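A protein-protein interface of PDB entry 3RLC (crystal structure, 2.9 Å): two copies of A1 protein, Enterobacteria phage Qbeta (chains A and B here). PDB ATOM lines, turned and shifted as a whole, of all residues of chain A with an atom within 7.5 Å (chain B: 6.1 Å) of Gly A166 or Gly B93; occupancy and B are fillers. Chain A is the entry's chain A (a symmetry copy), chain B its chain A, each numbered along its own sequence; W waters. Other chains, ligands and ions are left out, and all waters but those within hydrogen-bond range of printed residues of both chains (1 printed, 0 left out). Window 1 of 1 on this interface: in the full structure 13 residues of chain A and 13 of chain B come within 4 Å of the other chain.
Among the printed residues, 10 pairs touch across the chains.
Asn B94 touches its own counterpart, Asn A94.
2 positions are printed for both chains.
The backbone NH (N) of Lys B75 sits at hydrogen-bond distance from the backbone carbonyl oxygen (O) of Pro A163 (2.9 Å).
N of Gly A166 lies within hydrogen-bond range of O of Lys B75 (3.0 Å).
The backbone carbonyl oxygen (O) of Cys B91 lies within hydrogen-bond range of the side-chain hydroxyl (OG1) of Thr B74, at 2.6 Å.
The guanidinium group (NH2) of Arg B77 lies close to the backbone carbonyl oxygen (O) of Ile B169 (3.3 Å).
N of Gly B93 sits close to SG of Cys B91, at 3.4 Å.
Water W1 lies within hydrogen-bond range of the backbone carbonyl oxygen (O) of Gly A166 (2.7 Å), the backbone carbonyl oxygen (O) of Tyr B96 (2.8 Å) and the backbone NH (N) of Gly B95 (2.9 Å).
Gly A166 touches just these residues of chain B: Thr B74, Lys B75 and Gly B93.
Gly B93 touches just one residue of chain A: Gly A166 (3.7 Å).
Of the printed residues of chain B, Asn A94 touches Asn B94.
Printed residues of chain A within 4 Å of Thr B74: Ile A19 (3.7 Å), Pro A163 (3.6 Å), Gly A166 (3.3 Å) and Gly A167 (3.6 Å).
Printed residues of chain B within 4 Å of Gly A167: Thr B74.
Printed residues of chain A within 4 Å of Lys B75: Pro A163 (2.9 Å) and Gly A166 (3.0 Å).
Ile B169 touches none of the printed residues of chain A.
The nearest residue of chain B that does not touch Gly A166 is Ile B97 (4.3 Å).
Thr B74 touches Ile A19.
Asn A94 touches Asn B94 (OD1 to OD1, 3.6 Å).
Pro A163 touches Thr B74 (O to CA, 3.6 Å).
Arg B77 touches Ser A165 (NE to CB, 3.4 Å).
CA of Gly A166 touches OG1 of Thr B74, 3.3 Å away.
Gly A166 touches Gly B93 (O to CA, 3.7 Å).
Thr B74 touches Gly A167 (CG2 to N, 3.6 Å).
Arg B77 touches Ala A168 (NH2 to CB, 3.7 Å).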
ATOM      1  N   ILE A  19       1.080  11.750  -1.016  1.00  0.00           N
ATOM      2  CA  ILE A  19       1.013  11.068  -2.302  1.00  0.00           C
ATOM      3  C   ILE A  19       1.593   9.667  -2.205  1.00  0.00           C
ATOM      4  O   ILE A  19       2.704   9.494  -1.733  1.00  0.00           O
ATOM      5  CB  ILE A  19       1.755  11.868  -3.381  1.00  0.00           C
ATOM      6  CG1 ILE A  19       0.928  13.105  -3.768  1.00  0.00           C
ATOM      7  CG2 ILE A  19       2.042  10.996  -4.592  1.00  0.00           C
ATOM      8  CD1 ILE A  19       1.755  14.342  -4.071  1.00  0.00           C
ATOM      9  N   ASN A  94       8.892  10.778 -11.883  1.00  0.00           N
ATOM     10  CA  ASN A  94       7.524  10.707 -11.381  1.00  0.00           C
ATOM     11  C   ASN A  94       7.505  10.762  -9.857  1.00  0.00           C
ATOM     12  O   ASN A  94       6.598  10.202  -9.230  1.00  0.00           O
ATOM     13  CB  ASN A  94       6.855   9.391 -11.817  1.00  0.00           C
ATOM     14  CG  ASN A  94       6.408   9.395 -13.285  1.00  0.00           C
ATOM     15  OD1 ASN A  94       6.242  10.456 -13.908  1.00  0.00           O
ATOM     16  ND2 ASN A  94       6.189   8.188 -13.836  1.00  0.00           N
ATOM     17  N   TRP A 160       9.470  10.834  -3.379  1.00  0.00           N
ATOM     18  CA  TRP A 160       9.122  12.140  -2.839  1.00  0.00           C
ATOM     19  C   TRP A 160       7.618  12.346  -2.825  1.00  0.00           C
ATOM     20  O   TRP A 160       6.963  12.232  -3.847  1.00  0.00           O
ATOM     21  CB  TRP A 160       9.797  13.283  -3.606  1.00  0.00           C
ATOM     22  CG  TRP A 160       9.491  14.611  -2.957  1.00  0.00           C
ATOM     23  CD1 TRP A 160       8.437  15.432  -3.230  1.00  0.00           C
ATOM     24  CD2 TRP A 160      10.213  15.228  -1.887  1.00  0.00           C
ATOM     25  NE1 TRP A 160       8.468  16.536  -2.412  1.00  0.00           N
ATOM     26  CE2 TRP A 160       9.553  16.442  -1.581  1.00  0.00           C
ATOM     27  CE3 TRP A 160      11.358  14.878  -1.161  1.00  0.00           C
ATOM     28  CZ2 TRP A 160       9.999  17.312  -0.577  1.00  0.00           C
ATOM     29  CZ3 TRP A 160      11.806  15.738  -0.166  1.00  0.00           C
ATOM     30  CH2 TRP A 160      11.124  16.945   0.119  1.00  0.00           C
ATOM     31  N   ASP A 162       5.858  14.917  -0.635  1.00  0.00           N
ATOM     32  CA  ASP A 162       5.357  16.235  -0.236  1.00  0.00           C
ATOM     33  C   ASP A 162       4.701  16.845  -1.478  1.00  0.00           C
ATOM     34  O   ASP A 162       5.372  16.978  -2.512  1.00  0.00           O
ATOM     35  CB  ASP A 162       6.500  17.134   0.255  1.00  0.00           C
ATOM     36  CG  ASP A 162       6.006  18.329   1.063  1.00  0.00           C
ATOM     37  OD1 ASP A 162       4.789  18.491   1.213  1.00  0.00           O
ATOM     38  OD2 ASP A 162       6.826  19.125   1.568  1.00  0.00           O
ATOM     39  N   PRO A 163       3.395  17.201  -1.398  1.00  0.00           N
ATOM     40  CA  PRO A 163       2.673  17.774  -2.557  1.00  0.00           C
ATOM     41  C   PRO A 163       3.082  19.196  -3.007  1.00  0.00           C
ATOM     42  O   PRO A 163       2.750  19.600  -4.130  1.00  0.00           O
ATOM     43  CB  PRO A 163       1.206  17.740  -2.110  1.00  0.00           C
ATOM     44  CG  PRO A 163       1.279  17.812  -0.631  1.00  0.00           C
ATOM     45  CD  PRO A 163       2.489  16.996  -0.251  1.00  0.00           C
ATOM     46  N   SER A 164       3.800  19.944  -2.170  1.00  0.00           N
ATOM     47  CA  SER A 164       4.317  21.263  -2.583  1.00  0.00           C
ATOM     48  C   SER A 164       5.038  21.232  -3.936  1.00  0.00           C
ATOM     49  O   SER A 164       5.833  20.322  -4.224  1.00  0.00           O
ATOM     50  CB  SER A 164       5.250  21.855  -1.532  1.00  0.00           C
ATOM     51  OG  SER A 164       4.673  21.759  -0.239  1.00  0.00           O
ATOM     52  N   SER A 165       4.716  22.231  -4.763  1.00  0.00           N
ATOM     53  CA  SER A 165       5.395  22.510  -6.041  1.00  0.00           C
ATOM     54  C   SER A 165       5.213  21.416  -7.088  1.00  0.00           C
ATOM     55  O   SER A 165       6.167  21.009  -7.758  1.00  0.00           O
ATOM     56  CB  SER A 165       6.895  22.820  -5.816  1.00  0.00           C
ATOM     57  OG  SER A 165       7.099  23.849  -4.844  1.00  0.00           O
ATOM     58  N   GLY A 166       3.978  20.943  -7.233  1.00  0.00           N
ATOM     59  CA  GLY A 166       3.670  19.878  -8.201  1.00  0.00           C
ATOM     60  C   GLY A 166       4.558  18.647  -8.032  1.00  0.00           C
ATOM     61  O   GLY A 166       4.940  18.014  -9.021  1.00  0.00           O
ATOM     62  N   GLY A 167       4.875  18.319  -6.775  1.00  0.00           N
ATOM     63  CA  GLY A 167       5.809  17.249  -6.438  1.00  0.00           C
ATOM     64  C   GLY A 167       7.283  17.536  -6.750  1.00  0.00           C
ATOM     65  O   GLY A 167       8.077  16.573  -6.862  1.00  0.00           O
ATOM     66  N   ALA A 168       7.655  18.826  -6.902  1.00  0.00           N
ATOM     67  CA  ALA A 168       9.056  19.236  -7.178  1.00  0.00           C
ATOM     68  C   ALA A 168       9.984  19.096  -5.963  1.00  0.00           C
ATOM     69  O   ALA A 168       9.625  19.468  -4.838  1.00  0.00           O
ATOM     70  CB  ALA A 168       9.133  20.639  -7.751  1.00  0.00           C
ATOM     71  N   ILE A 169      11.185  18.582  -6.225  1.00  0.00           N
ATOM     72  CA  ILE A 169      12.084  18.046  -5.207  1.00  0.00           C
ATOM     73  C   ILE A 169      13.131  19.089  -4.800  1.00  0.00           C
ATOM     74  O   ILE A 169      13.884  19.546  -5.645  1.00  0.00           O
ATOM     75  CB  ILE A 169      12.747  16.726  -5.735  1.00  0.00           C
ATOM     76  CG1 ILE A 169      11.693  15.610  -5.835  1.00  0.00           C
ATOM     77  CG2 ILE A 169      13.877  16.265  -4.836  1.00  0.00           C
ATOM     78  CD1 ILE A 169      11.836  14.678  -7.023  1.00  0.00           C
ATOM     79  N   LEU B  70      -4.677  16.822 -16.308  1.00  0.00           N
ATOM     80  CA  LEU B  70      -3.774  17.823 -15.816  1.00  0.00           C
ATOM     81  C   LEU B  70      -4.012  18.019 -14.344  1.00  0.00           C
ATOM     82  O   LEU B  70      -3.269  18.754 -13.693  1.00  0.00           O
ATOM     83  CB  LEU B  70      -3.990  19.131 -16.569  1.00  0.00           C
ATOM     84  CG  LEU B  70      -4.256  19.025 -18.073  1.00  0.00           C
ATOM     85  CD1 LEU B  70      -4.557  20.371 -18.643  1.00  0.00           C
ATOM     86  CD2 LEU B  70      -3.084  18.422 -18.825  1.00  0.00           C
ATOM     87  N   LEU B  71      -5.033  17.364 -13.807  1.00  0.00           N
ATOM     88  CA  LEU B  71      -5.327  17.493 -12.385  1.00  0.00           C
ATOM     89  C   LEU B  71      -4.818  16.317 -11.586  1.00  0.00           C
ATOM     90  O   LEU B  71      -4.569  15.239 -12.118  1.00  0.00           O
ATOM     91  CB  LEU B  71      -6.815  17.650 -12.156  1.00  0.00           C
ATOM     92  CG  LEU B  71      -7.494  18.767 -12.937  1.00  0.00           C
ATOM     93  CD1 LEU B  71      -8.871  18.954 -12.372  1.00  0.00           C
ATOM     94  CD2 LEU B  71      -6.694  20.068 -12.843  1.00  0.00           C
ATOM     95  N   GLY B  72      -4.654  16.528 -10.298  1.00  0.00           N
ATOM     96  CA  GLY B  72      -4.111  15.506  -9.418  1.00  0.00           C
ATOM     97  C   GLY B  72      -4.085  16.176  -8.075  1.00  0.00           C
ATOM     98  O   GLY B  72      -4.809  17.141  -7.863  1.00  0.00           O
ATOM     99  N   THR B  74      -1.095  17.324  -6.299  1.00  0.00           N
ATOM    100  CA  THR B  74       0.073  18.152  -5.966  1.00  0.00           C
ATOM    101  C   THR B  74      -0.387  19.613  -5.957  1.00  0.00           C
ATOM    102  O   THR B  74      -1.216  19.985  -6.773  1.00  0.00           O
ATOM    103  CB  THR B  74       1.227  17.975  -6.985  1.00  0.00           C
ATOM    104  OG1 THR B  74       0.768  18.293  -8.298  1.00  0.00           O
ATOM    105  CG2 THR B  74       1.751  16.563  -7.000  1.00  0.00           C
ATOM    106  N   LYS B  75       0.110  20.434  -5.039  1.00  0.00           N
ATOM    107  CA  LYS B  75      -0.254  21.859  -5.041  1.00  0.00           C
ATOM    108  C   LYS B  75       0.266  22.547  -6.312  1.00  0.00           C
ATOM    109  O   LYS B  75       1.283  22.133  -6.863  1.00  0.00           O
ATOM    110  CB  LYS B  75       0.287  22.573  -3.798  1.00  0.00           C
ATOM    111  CG  LYS B  75      -0.340  22.111  -2.471  1.00  0.00           C
ATOM    112  CD  LYS B  75      -0.510  23.294  -1.470  1.00  0.00           C
ATOM    113  CE  LYS B  75       0.839  23.824  -0.890  1.00  0.00           C
ATOM    114  NZ  LYS B  75       0.639  24.890   0.158  1.00  0.00           N
ATOM    115  N   TRP B  76      -0.427  23.575  -6.799  1.00  0.00           N
ATOM    116  CA  TRP B  76       0.100  24.360  -7.932  1.00  0.00           C
ATOM    117  C   TRP B  76       1.236  25.260  -7.460  1.00  0.00           C
ATOM    118  O   TRP B  76       1.263  25.671  -6.300  1.00  0.00           O
ATOM    119  CB  TRP B  76      -0.988  25.215  -8.575  1.00  0.00           C
ATOM    120  CG  TRP B  76      -2.078  24.410  -9.131  1.00  0.00           C
ATOM    121  CD1 TRP B  76      -3.258  24.102  -8.523  1.00  0.00           C
ATOM    122  CD2 TRP B  76      -2.102  23.781 -10.417  1.00  0.00           C
ATOM    123  NE1 TRP B  76      -4.023  23.304  -9.350  1.00  0.00           N
ATOM    124  CE2 TRP B  76      -3.335  23.092 -10.520  1.00  0.00           C
ATOM    125  CE3 TRP B  76      -1.202  23.729 -11.493  1.00  0.00           C
ATOM    126  CZ2 TRP B  76      -3.695  22.360 -11.666  1.00  0.00           C
ATOM    127  CZ3 TRP B  76      -1.552  22.999 -12.625  1.00  0.00           C
ATOM    128  CH2 TRP B  76      -2.787  22.320 -12.699  1.00  0.00           C
ATOM    129  N   ARG B  77       2.168  25.584  -8.343  1.00  0.00           N
ATOM    130  CA  ARG B  77       3.211  26.510  -7.964  1.00  0.00           C
ATOM    131  C   ARG B  77       2.598  27.860  -7.578  1.00  0.00           C
ATOM    132  O   ARG B  77       2.986  28.443  -6.569  1.00  0.00           O
ATOM    133  CB  ARG B  77       4.240  26.651  -9.067  1.00  0.00           C
ATOM    134  CG  ARG B  77       5.505  27.322  -8.610  1.00  0.00           C
ATOM    135  CD  ARG B  77       6.269  26.513  -7.556  1.00  0.00           C
ATOM    136  NE  ARG B  77       6.945  25.320  -8.102  1.00  0.00           N
ATOM    137  CZ  ARG B  77       8.251  25.244  -8.415  1.00  0.00           C
ATOM    138  NH1 ARG B  77       9.058  26.300  -8.270  1.00  0.00           N
ATOM    139  NH2 ARG B  77       8.758  24.103  -8.886  1.00  0.00           N
ATOM    140  N   CYS B  91      -2.767  19.822  -8.964  1.00  0.00           N
ATOM    141  CA  CYS B  91      -2.055  19.508 -10.202  1.00  0.00           C
ATOM    142  C   CYS B  91      -1.707  18.034 -10.285  1.00  0.00           C
ATOM    143  O   CYS B  91      -1.419  17.396  -9.264  1.00  0.00           O
ATOM    144  CB  CYS B  91      -0.775  20.332 -10.273  1.00  0.00           C
ATOM    145  SG  CYS B  91       0.208  20.063 -11.747  1.00  0.00           S
ATOM    146  N   ARG B  92      -1.718  17.518 -11.514  1.00  0.00           N
ATOM    147  CA  ARG B  92      -1.358  16.138 -11.802  1.00  0.00           C
ATOM    148  C   ARG B  92       0.087  15.819 -11.408  1.00  0.00           C
ATOM    149  O   ARG B  92       0.387  14.710 -10.959  1.00  0.00           O
ATOM    150  CB  ARG B  92      -1.616  15.836 -13.279  1.00  0.00           C
ATOM    151  CG  ARG B  92      -0.752  14.748 -13.881  1.00  0.00           C
ATOM    152  CD  ARG B  92      -1.080  13.388 -13.360  1.00  0.00           C
ATOM    153  NE  ARG B  92      -2.370  12.936 -13.849  1.00  0.00           N
ATOM    154  CZ  ARG B  92      -2.810  11.676 -13.749  1.00  0.00           C
ATOM    155  NH1 ARG B  92      -2.040  10.738 -13.174  1.00  0.00           N
ATOM    156  NH2 ARG B  92      -4.021  11.341 -14.227  1.00  0.00           N
ATOM    157  N   GLY B  93       0.984  16.783 -11.569  1.00  0.00           N
ATOM    158  CA  GLY B  93       2.373  16.558 -11.200  1.00  0.00           C
ATOM    159  C   GLY B  93       2.977  15.672 -12.266  1.00  0.00           C
ATOM    160  O   GLY B  93       2.715  15.884 -13.458  1.00  0.00           O
ATOM    161  N   ASN B  94       3.762  14.668 -11.863  1.00  0.00           N
ATOM    162  CA  ASN B  94       4.411  13.792 -12.834  1.00  0.00           C
ATOM    163  C   ASN B  94       5.091  14.610 -13.925  1.00  0.00           C
ATOM    164  O   ASN B  94       5.215  14.138 -15.063  1.00  0.00           O
ATOM    165  CB  ASN B  94       3.377  12.869 -13.504  1.00  0.00           C
ATOM    166  CG  ASN B  94       2.938  11.700 -12.613  1.00  0.00           C
ATOM    167  OD1 ASN B  94       3.626  11.327 -11.649  1.00  0.00           O
ATOM    168  ND2 ASN B  94       1.784  11.100 -12.956  1.00  0.00           N
ATOM    169  N   GLY B  95       5.485  15.843 -13.598  1.00  0.00           N
ATOM    170  CA  GLY B  95       6.096  16.760 -14.569  1.00  0.00           C
ATOM    171  C   GLY B  95       5.238  17.903 -15.112  1.00  0.00           C
ATOM    172  O   GLY B  95       5.771  18.839 -15.709  1.00  0.00           O
ATOM    173  N   TYR B  96       3.917  17.823 -14.943  1.00  0.00           N
ATOM    174  CA  TYR B  96       3.033  18.941 -15.251  1.00  0.00           C
ATOM    175  C   TYR B  96       3.192  19.998 -14.166  1.00  0.00           C
ATOM    176  O   TYR B  96       3.354  19.679 -12.983  1.00  0.00           O
ATOM    177  CB  TYR B  96       1.560  18.515 -15.305  1.00  0.00           C
ATOM    178  CG  TYR B  96       1.150  17.689 -16.512  1.00  0.00           C
ATOM    179  CD1 TYR B  96       1.008  18.273 -17.770  1.00  0.00           C
ATOM    180  CD2 TYR B  96       0.871  16.326 -16.386  1.00  0.00           C
ATOM    181  CE1 TYR B  96       0.619  17.523 -18.885  1.00  0.00           C
ATOM    182  CE2 TYR B  96       0.479  15.566 -17.491  1.00  0.00           C
ATOM    183  CZ  TYR B  96       0.362  16.176 -18.738  1.00  0.00           C
ATOM    184  OH  TYR B  96      -0.019  15.438 -19.831  1.00  0.00           O
ATOM    185  N   ILE B  97       3.130  21.260 -14.574  1.00  0.00           N
ATOM    186  CA  ILE B  97       3.326  22.375 -13.662  1.00  0.00           C
ATOM    187  C   ILE B  97       2.757  23.648 -14.297  1.00  0.00           C
ATOM    188  O   ILE B  97       2.969  23.897 -15.477  1.00  0.00           O
ATOM    189  CB  ILE B  97       4.828  22.533 -13.297  1.00  0.00           C
ATOM    190  CG1 ILE B  97       5.034  23.551 -12.183  1.00  0.00           C
ATOM    191  CG2 ILE B  97       5.653  22.950 -14.515  1.00  0.00           C
ATOM    192  CD1 ILE B  97       4.420  23.143 -10.852  1.00  0.00           C
ATOM    193  N   PHE B 159       4.519  21.246 -19.487  1.00  0.00           N
ATOM    194  CA  PHE B 159       5.056  19.964 -19.081  1.00  0.00           C
ATOM    195  C   PHE B 159       6.560  20.037 -18.994  1.00  0.00           C
ATOM    196  O   PHE B 159       7.230  20.320 -19.984  1.00  0.00           O
ATOM    197  CB  PHE B 159       4.649  18.836 -20.033  1.00  0.00           C
ATOM    198  CG  PHE B 159       5.162  17.495 -19.594  1.00  0.00           C
ATOM    199  CD1 PHE B 159       4.521  16.790 -18.565  1.00  0.00           C
ATOM    200  CD2 PHE B 159       6.318  16.958 -20.152  1.00  0.00           C
ATOM    201  CE1 PHE B 159       5.026  15.561 -18.107  1.00  0.00           C
ATOM    202  CE2 PHE B 159       6.832  15.731 -19.700  1.00  0.00           C
ATOM    203  CZ  PHE B 159       6.193  15.036 -18.683  1.00  0.00           C
ATOM    204  N   ILE B 169      11.766  20.413 -10.820  1.00  0.00           N
ATOM    205  CA  ILE B 169      11.410  21.664 -11.485  1.00  0.00           C
ATOM    206  C   ILE B 169      12.064  22.859 -10.784  1.00  0.00           C
ATOM    207  O   ILE B 169      11.822  23.074  -9.607  1.00  0.00           O
ATOM    208  CB  ILE B 169       9.848  21.801 -11.542  1.00  0.00           C
ATOM    209  CG1 ILE B 169       9.262  20.759 -12.509  1.00  0.00           C
ATOM    210  CG2 ILE B 169       9.422  23.186 -11.984  1.00  0.00           C
ATOM    211  CD1 ILE B 169       7.942  20.142 -12.087  1.00  0.00           C
HETATM  212  O   HOH W   1       5.260  18.039 -11.701  1.00  0.00           O
